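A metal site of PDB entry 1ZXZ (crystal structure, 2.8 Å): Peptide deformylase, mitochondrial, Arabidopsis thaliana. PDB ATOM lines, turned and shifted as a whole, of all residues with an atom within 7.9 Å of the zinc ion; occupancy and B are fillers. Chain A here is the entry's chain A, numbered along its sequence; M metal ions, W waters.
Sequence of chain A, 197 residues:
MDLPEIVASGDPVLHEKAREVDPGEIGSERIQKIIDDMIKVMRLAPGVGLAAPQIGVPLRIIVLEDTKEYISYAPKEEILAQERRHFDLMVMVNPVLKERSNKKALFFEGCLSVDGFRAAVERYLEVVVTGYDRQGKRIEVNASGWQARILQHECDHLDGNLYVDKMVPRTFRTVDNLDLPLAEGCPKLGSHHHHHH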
ATOM      1  N   LEU A  14      -9.927 -21.722   0.637  1.00  0.00           N
ATOM      2  CA  LEU A  14      -8.814 -22.387   1.276  1.00  0.00           C
ATOM      3  C   LEU A  14      -8.674 -21.894   2.709  1.00  0.00           C
ATOM      4  O   LEU A  14      -8.177 -22.620   3.575  1.00  0.00           O
ATOM      5  CB  LEU A  14      -7.535 -22.078   0.473  1.00  0.00           C
ATOM      6  CG  LEU A  14      -6.644 -23.216  -0.023  1.00  0.00           C
ATOM      7  CD1 LEU A  14      -7.460 -24.350  -0.598  1.00  0.00           C
ATOM      8  CD2 LEU A  14      -5.702 -22.667  -1.067  1.00  0.00           C
ATOM      9  N   GLY A  49      -2.383 -36.739   0.700  1.00  0.00           N
ATOM     10  CA  GLY A  49      -3.634 -36.246   1.267  1.00  0.00           C
ATOM     11  C   GLY A  49      -4.189 -35.102   0.449  1.00  0.00           C
ATOM     12  O   GLY A  49      -3.442 -34.373  -0.200  1.00  0.00           O
ATOM     13  N   LEU A  50      -5.502 -34.939   0.487  1.00  0.00           N
ATOM     14  CA  LEU A  50      -6.144 -33.881  -0.287  1.00  0.00           C
ATOM     15  C   LEU A  50      -7.494 -33.557   0.342  1.00  0.00           C
ATOM     16  O   LEU A  50      -8.235 -34.458   0.727  1.00  0.00           O
ATOM     17  CB  LEU A  50      -6.349 -34.373  -1.734  1.00  0.00           C
ATOM     18  CG  LEU A  50      -6.279 -33.415  -2.932  1.00  0.00           C
ATOM     19  CD1 LEU A  50      -7.566 -32.683  -3.067  1.00  0.00           C
ATOM     20  CD2 LEU A  50      -5.124 -32.451  -2.796  1.00  0.00           C
ATOM     21  N   ALA A  51      -7.794 -32.270   0.475  1.00  0.00           N
ATOM     22  CA  ALA A  51      -9.077 -31.861   1.048  1.00  0.00           C
ATOM     23  C   ALA A  51      -9.893 -31.119  -0.003  1.00  0.00           C
ATOM     24  O   ALA A  51      -9.346 -30.374  -0.815  1.00  0.00           O
ATOM     25  CB  ALA A  51      -8.848 -30.972   2.248  1.00  0.00           C
ATOM     26  N   GLN A  54      -9.276 -27.771  -1.554  1.00  0.00           N
ATOM     27  CA  GLN A  54      -8.115 -27.726  -2.433  1.00  0.00           C
ATOM     28  C   GLN A  54      -8.410 -27.855  -3.911  1.00  0.00           C
ATOM     29  O   GLN A  54      -7.498 -27.768  -4.743  1.00  0.00           O
ATOM     30  CB  GLN A  54      -7.070 -28.759  -1.998  1.00  0.00           C
ATOM     31  CG  GLN A  54      -6.112 -28.178  -0.990  1.00  0.00           C
ATOM     32  CD  GLN A  54      -4.953 -29.091  -0.670  1.00  0.00           C
ATOM     33  OE1 GLN A  54      -5.099 -30.081   0.046  1.00  0.00           O
ATOM     34  NE2 GLN A  54      -3.787 -28.752  -1.206  1.00  0.00           N
ATOM     35  N   GLU A 109       6.417 -30.519   6.838  1.00  0.00           N
ATOM     36  CA  GLU A 109       5.178 -30.674   6.089  1.00  0.00           C
ATOM     37  C   GLU A 109       5.126 -29.780   4.863  1.00  0.00           C
ATOM     38  O   GLU A 109       5.774 -28.731   4.806  1.00  0.00           O
ATOM     39  CB  GLU A 109       3.958 -30.365   6.966  1.00  0.00           C
ATOM     40  CG  GLU A 109       3.367 -31.590   7.670  1.00  0.00           C
ATOM     41  CD  GLU A 109       2.089 -31.270   8.411  1.00  0.00           C
ATOM     42  OE1 GLU A 109       1.186 -30.672   7.779  1.00  0.00           O
ATOM     43  OE2 GLU A 109       1.982 -31.623   9.600  1.00  0.00           O
ATOM     44  N   GLY A 110       4.358 -30.220   3.878  1.00  0.00           N
ATOM     45  CA  GLY A 110       4.208 -29.449   2.675  1.00  0.00           C
ATOM     46  C   GLY A 110       2.761 -29.530   2.299  1.00  0.00           C
ATOM     47  O   GLY A 110       1.985 -30.297   2.872  1.00  0.00           O
ATOM     48  N   CYS A 111       2.385 -28.711   1.332  1.00  0.00           N
ATOM     49  CA  CYS A 111       1.020 -28.710   0.853  1.00  0.00           C
ATOM     50  C   CYS A 111       1.052 -28.371  -0.611  1.00  0.00           C
ATOM     51  O   CYS A 111       1.874 -27.558  -1.059  1.00  0.00           O
ATOM     52  CB  CYS A 111       0.188 -27.681   1.601  1.00  0.00           C
ATOM     53  SG  CYS A 111      -1.487 -27.629   0.972  1.00  0.00           S
ATOM     54  N   LEU A 112       0.178 -29.012  -1.378  1.00  0.00           N
ATOM     55  CA  LEU A 112       0.115 -28.763  -2.801  1.00  0.00           C
ATOM     56  C   LEU A 112      -0.424 -27.365  -3.086  1.00  0.00           C
ATOM     57  O   LEU A 112      -0.354 -26.872  -4.212  1.00  0.00           O
ATOM     58  CB  LEU A 112      -0.724 -29.838  -3.471  1.00  0.00           C
ATOM     59  CG  LEU A 112       0.154 -30.746  -4.334  1.00  0.00           C
ATOM     60  CD1 LEU A 112      -0.436 -32.136  -4.449  1.00  0.00           C
ATOM     61  CD2 LEU A 112       0.329 -30.108  -5.706  1.00  0.00           C
ATOM     62  N   SER A 113      -0.950 -26.714  -2.046  1.00  0.00           N
ATOM     63  CA  SER A 113      -1.474 -25.361  -2.194  1.00  0.00           C
ATOM     64  C   SER A 113      -0.401 -24.309  -1.952  1.00  0.00           C
ATOM     65  O   SER A 113      -0.639 -23.122  -2.194  1.00  0.00           O
ATOM     66  CB  SER A 113      -2.653 -25.134  -1.249  1.00  0.00           C
ATOM     67  OG  SER A 113      -3.780 -25.886  -1.664  1.00  0.00           O
ATOM     68  N   VAL A 114       0.766 -24.742  -1.474  1.00  0.00           N
ATOM     69  CA  VAL A 114       1.945 -23.891  -1.241  1.00  0.00           C
ATOM     70  C   VAL A 114       3.126 -24.756  -1.642  1.00  0.00           C
ATOM     71  O   VAL A 114       3.713 -25.457  -0.810  1.00  0.00           O
ATOM     72  CB  VAL A 114       2.196 -23.517   0.235  1.00  0.00           C
ATOM     73  CG1 VAL A 114       3.230 -22.415   0.290  1.00  0.00           C
ATOM     74  CG2 VAL A 114       0.924 -23.110   0.934  1.00  0.00           C
ATOM     75  N   ARG A 123       2.531 -32.134  15.385  1.00  0.00           N
ATOM     76  CA  ARG A 123       1.289 -32.874  15.236  1.00  0.00           C
ATOM     77  C   ARG A 123       1.143 -33.906  16.342  1.00  0.00           C
ATOM     78  O   ARG A 123       2.131 -34.334  16.917  1.00  0.00           O
ATOM     79  CB  ARG A 123       1.260 -33.587  13.889  1.00  0.00           C
ATOM     80  CG  ARG A 123       1.274 -32.686  12.658  1.00  0.00           C
ATOM     81  CD  ARG A 123       0.001 -31.862  12.485  1.00  0.00           C
ATOM     82  NE  ARG A 123      -0.027 -31.144  11.218  1.00  0.00           N
ATOM     83  CZ  ARG A 123      -0.912 -30.184  10.939  1.00  0.00           C
ATOM     84  NH1 ARG A 123      -1.802 -29.855  11.861  1.00  0.00           N
ATOM     85  NH2 ARG A 123      -0.977 -29.622   9.737  1.00  0.00           N
ATOM     86  N   ILE A 150      -1.222 -36.839   8.351  1.00  0.00           N
ATOM     87  CA  ILE A 150      -1.951 -36.533   7.140  1.00  0.00           C
ATOM     88  C   ILE A 150      -3.381 -36.155   7.522  1.00  0.00           C
ATOM     89  O   ILE A 150      -3.934 -35.154   7.048  1.00  0.00           O
ATOM     90  CB  ILE A 150      -1.973 -37.745   6.178  1.00  0.00           C
ATOM     91  CG1 ILE A 150      -0.529 -38.132   5.799  1.00  0.00           C
ATOM     92  CG2 ILE A 150      -2.783 -37.391   4.931  1.00  0.00           C
ATOM     93  CD1 ILE A 150      -0.416 -39.290   4.794  1.00  0.00           C
ATOM     94  N   HIS A 153      -3.462 -32.622   8.976  1.00  0.00           N
ATOM     95  CA  HIS A 153      -3.192 -31.649   7.930  1.00  0.00           C
ATOM     96  C   HIS A 153      -4.433 -31.441   7.077  1.00  0.00           C
ATOM     97  O   HIS A 153      -4.871 -30.306   6.863  1.00  0.00           O
ATOM     98  CB  HIS A 153      -2.063 -32.140   7.028  1.00  0.00           C
ATOM     99  CG  HIS A 153      -1.830 -31.271   5.839  1.00  0.00           C
ATOM    100  ND1 HIS A 153      -0.789 -30.370   5.758  1.00  0.00           N
ATOM    101  CD2 HIS A 153      -2.537 -31.126   4.690  1.00  0.00           C
ATOM    102  CE1 HIS A 153      -0.865 -29.703   4.622  1.00  0.00           C
ATOM    103  NE2 HIS A 153      -1.915 -30.143   3.949  1.00  0.00           N
ATOM    104  N   GLU A 154      -4.994 -32.534   6.581  1.00  0.00           N
ATOM    105  CA  GLU A 154      -6.175 -32.462   5.736  1.00  0.00           C
ATOM    106  C   GLU A 154      -7.398 -31.900   6.455  1.00  0.00           C
ATOM    107  O   GLU A 154      -8.057 -31.009   5.931  1.00  0.00           O
ATOM    108  CB  GLU A 154      -6.504 -33.847   5.173  1.00  0.00           C
ATOM    109  CG  GLU A 154      -5.457 -34.384   4.196  1.00  0.00           C
ATOM    110  CD  GLU A 154      -5.130 -33.400   3.091  1.00  0.00           C
ATOM    111  OE1 GLU A 154      -6.027 -32.633   2.688  1.00  0.00           O
ATOM    112  OE2 GLU A 154      -3.981 -33.403   2.613  1.00  0.00           O
ATOM    113  N   ASP A 156      -7.462 -29.986   8.947  1.00  0.00           N
ATOM    114  CA  ASP A 156      -7.220 -28.560   9.150  1.00  0.00           C
ATOM    115  C   ASP A 156      -7.791 -27.801   7.970  1.00  0.00           C
ATOM    116  O   ASP A 156      -8.497 -26.807   8.124  1.00  0.00           O
ATOM    117  CB  ASP A 156      -5.730 -28.298   9.284  1.00  0.00           C
ATOM    118  CG  ASP A 156      -5.206 -28.586  10.666  1.00  0.00           C
ATOM    119  OD1 ASP A 156      -5.891 -29.325  11.395  1.00  0.00           O
ATOM    120  OD2 ASP A 156      -4.110 -28.097  11.019  1.00  0.00           O
ATOM    121  N   HIS A 157      -7.468 -28.282   6.767  1.00  0.00           N
ATOM    122  CA  HIS A 157      -7.950 -27.670   5.550  1.00  0.00           C
ATOM    123  C   HIS A 157      -9.457 -27.400   5.617  1.00  0.00           C
ATOM    124  O   HIS A 157      -9.936 -26.381   5.134  1.00  0.00           O
ATOM    125  CB  HIS A 157      -7.661 -28.578   4.362  1.00  0.00           C
ATOM    126  CG  HIS A 157      -6.312 -28.367   3.749  1.00  0.00           C
ATOM    127  ND1 HIS A 157      -5.961 -27.204   3.113  1.00  0.00           N
ATOM    128  CD2 HIS A 157      -5.236 -29.175   3.672  1.00  0.00           C
ATOM    129  CE1 HIS A 157      -4.724 -27.298   2.669  1.00  0.00           C
ATOM    130  NE2 HIS A 157      -4.258 -28.488   2.994  1.00  0.00           N
ATOM    131  N   ASN A 161      -7.469 -23.763   7.701  1.00  0.00           N
ATOM    132  CA  ASN A 161      -6.143 -23.571   8.285  1.00  0.00           C
ATOM    133  C   ASN A 161      -5.051 -24.271   7.492  1.00  0.00           C
ATOM    134  O   ASN A 161      -5.233 -25.409   7.054  1.00  0.00           O
ATOM    135  CB  ASN A 161      -6.148 -24.115   9.706  1.00  0.00           C
ATOM    136  CG  ASN A 161      -7.364 -23.689  10.457  1.00  0.00           C
ATOM    137  OD1 ASN A 161      -7.717 -22.506  10.465  1.00  0.00           O
ATOM    138  ND2 ASN A 161      -8.028 -24.645  11.104  1.00  0.00           N
ATOM    139  N   LEU A 162      -3.924 -23.588   7.302  1.00  0.00           N
ATOM    140  CA  LEU A 162      -2.795 -24.162   6.574  1.00  0.00           C
ATOM    141  C   LEU A 162      -1.594 -24.311   7.511  1.00  0.00           C
ATOM    142  O   LEU A 162      -1.503 -23.627   8.527  1.00  0.00           O
ATOM    143  CB  LEU A 162      -2.430 -23.272   5.367  1.00  0.00           C
ATOM    144  CG  LEU A 162      -3.543 -22.976   4.363  1.00  0.00           C
ATOM    145  CD1 LEU A 162      -2.955 -22.272   3.155  1.00  0.00           C
ATOM    146  CD2 LEU A 162      -4.227 -24.265   3.936  1.00  0.00           C
ATOM    147  N   TYR A 163      -0.665 -25.181   7.167  1.00  0.00           N
ATOM    148  CA  TYR A 163       0.475 -25.404   8.039  1.00  0.00           C
ATOM    149  C   TYR A 163       1.268 -24.138   8.321  1.00  0.00           C
ATOM    150  O   TYR A 163       1.714 -23.920   9.442  1.00  0.00           O
ATOM    151  CB  TYR A 163       1.399 -26.490   7.461  1.00  0.00           C
ATOM    152  CG  TYR A 163       2.238 -26.114   6.259  1.00  0.00           C
ATOM    153  CD1 TYR A 163       3.634 -26.051   6.365  1.00  0.00           C
ATOM    154  CD2 TYR A 163       1.665 -25.901   5.011  1.00  0.00           C
ATOM    155  CE1 TYR A 163       4.435 -25.800   5.259  1.00  0.00           C
ATOM    156  CE2 TYR A 163       2.448 -25.658   3.900  1.00  0.00           C
ATOM    157  CZ  TYR A 163       3.837 -25.614   4.017  1.00  0.00           C
ATOM    158  OH  TYR A 163       4.638 -25.425   2.890  1.00  0.00           O
HETATM  159 ZN    ZN M   1      -2.578 -29.372   2.192  1.00  0.00          ZN
HETATM  160  O   HOH W   1      -3.593 -31.100   1.680  1.00  0.00           O
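A ring nitrogen (ND1) of His 153 lies within hydrogen-bond range of the side-chain carboxylate of Glu 109.
OE1 of Gln 54 lies close to NE2 of His 157, at 3.5 Å.
SG of Cys 111 sits close to NE2 of Gln 54 (3.4 Å).
The backbone NH (N) of Ser 113 lies close to the side-chain sulfur (SG) of Cys 111 (3.2 Å).
OG of Ser 113 is in hydrogen-bond range of NE2 of Gln 54 (2.9 Å).
N of Ala 51 is in hydrogen-bond range of OE1 of Gln 54 (3.5 Å).
Gln 54 touches the zinc ion.
The zinc ion is bound by NE2 of His 153, NE2 of His 157, water W1 and SG of Cys 111.
Water W1 bridges OE1 of Gln 54 (2.4 Å) and OE2 of Glu 154 (2.5 Å).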
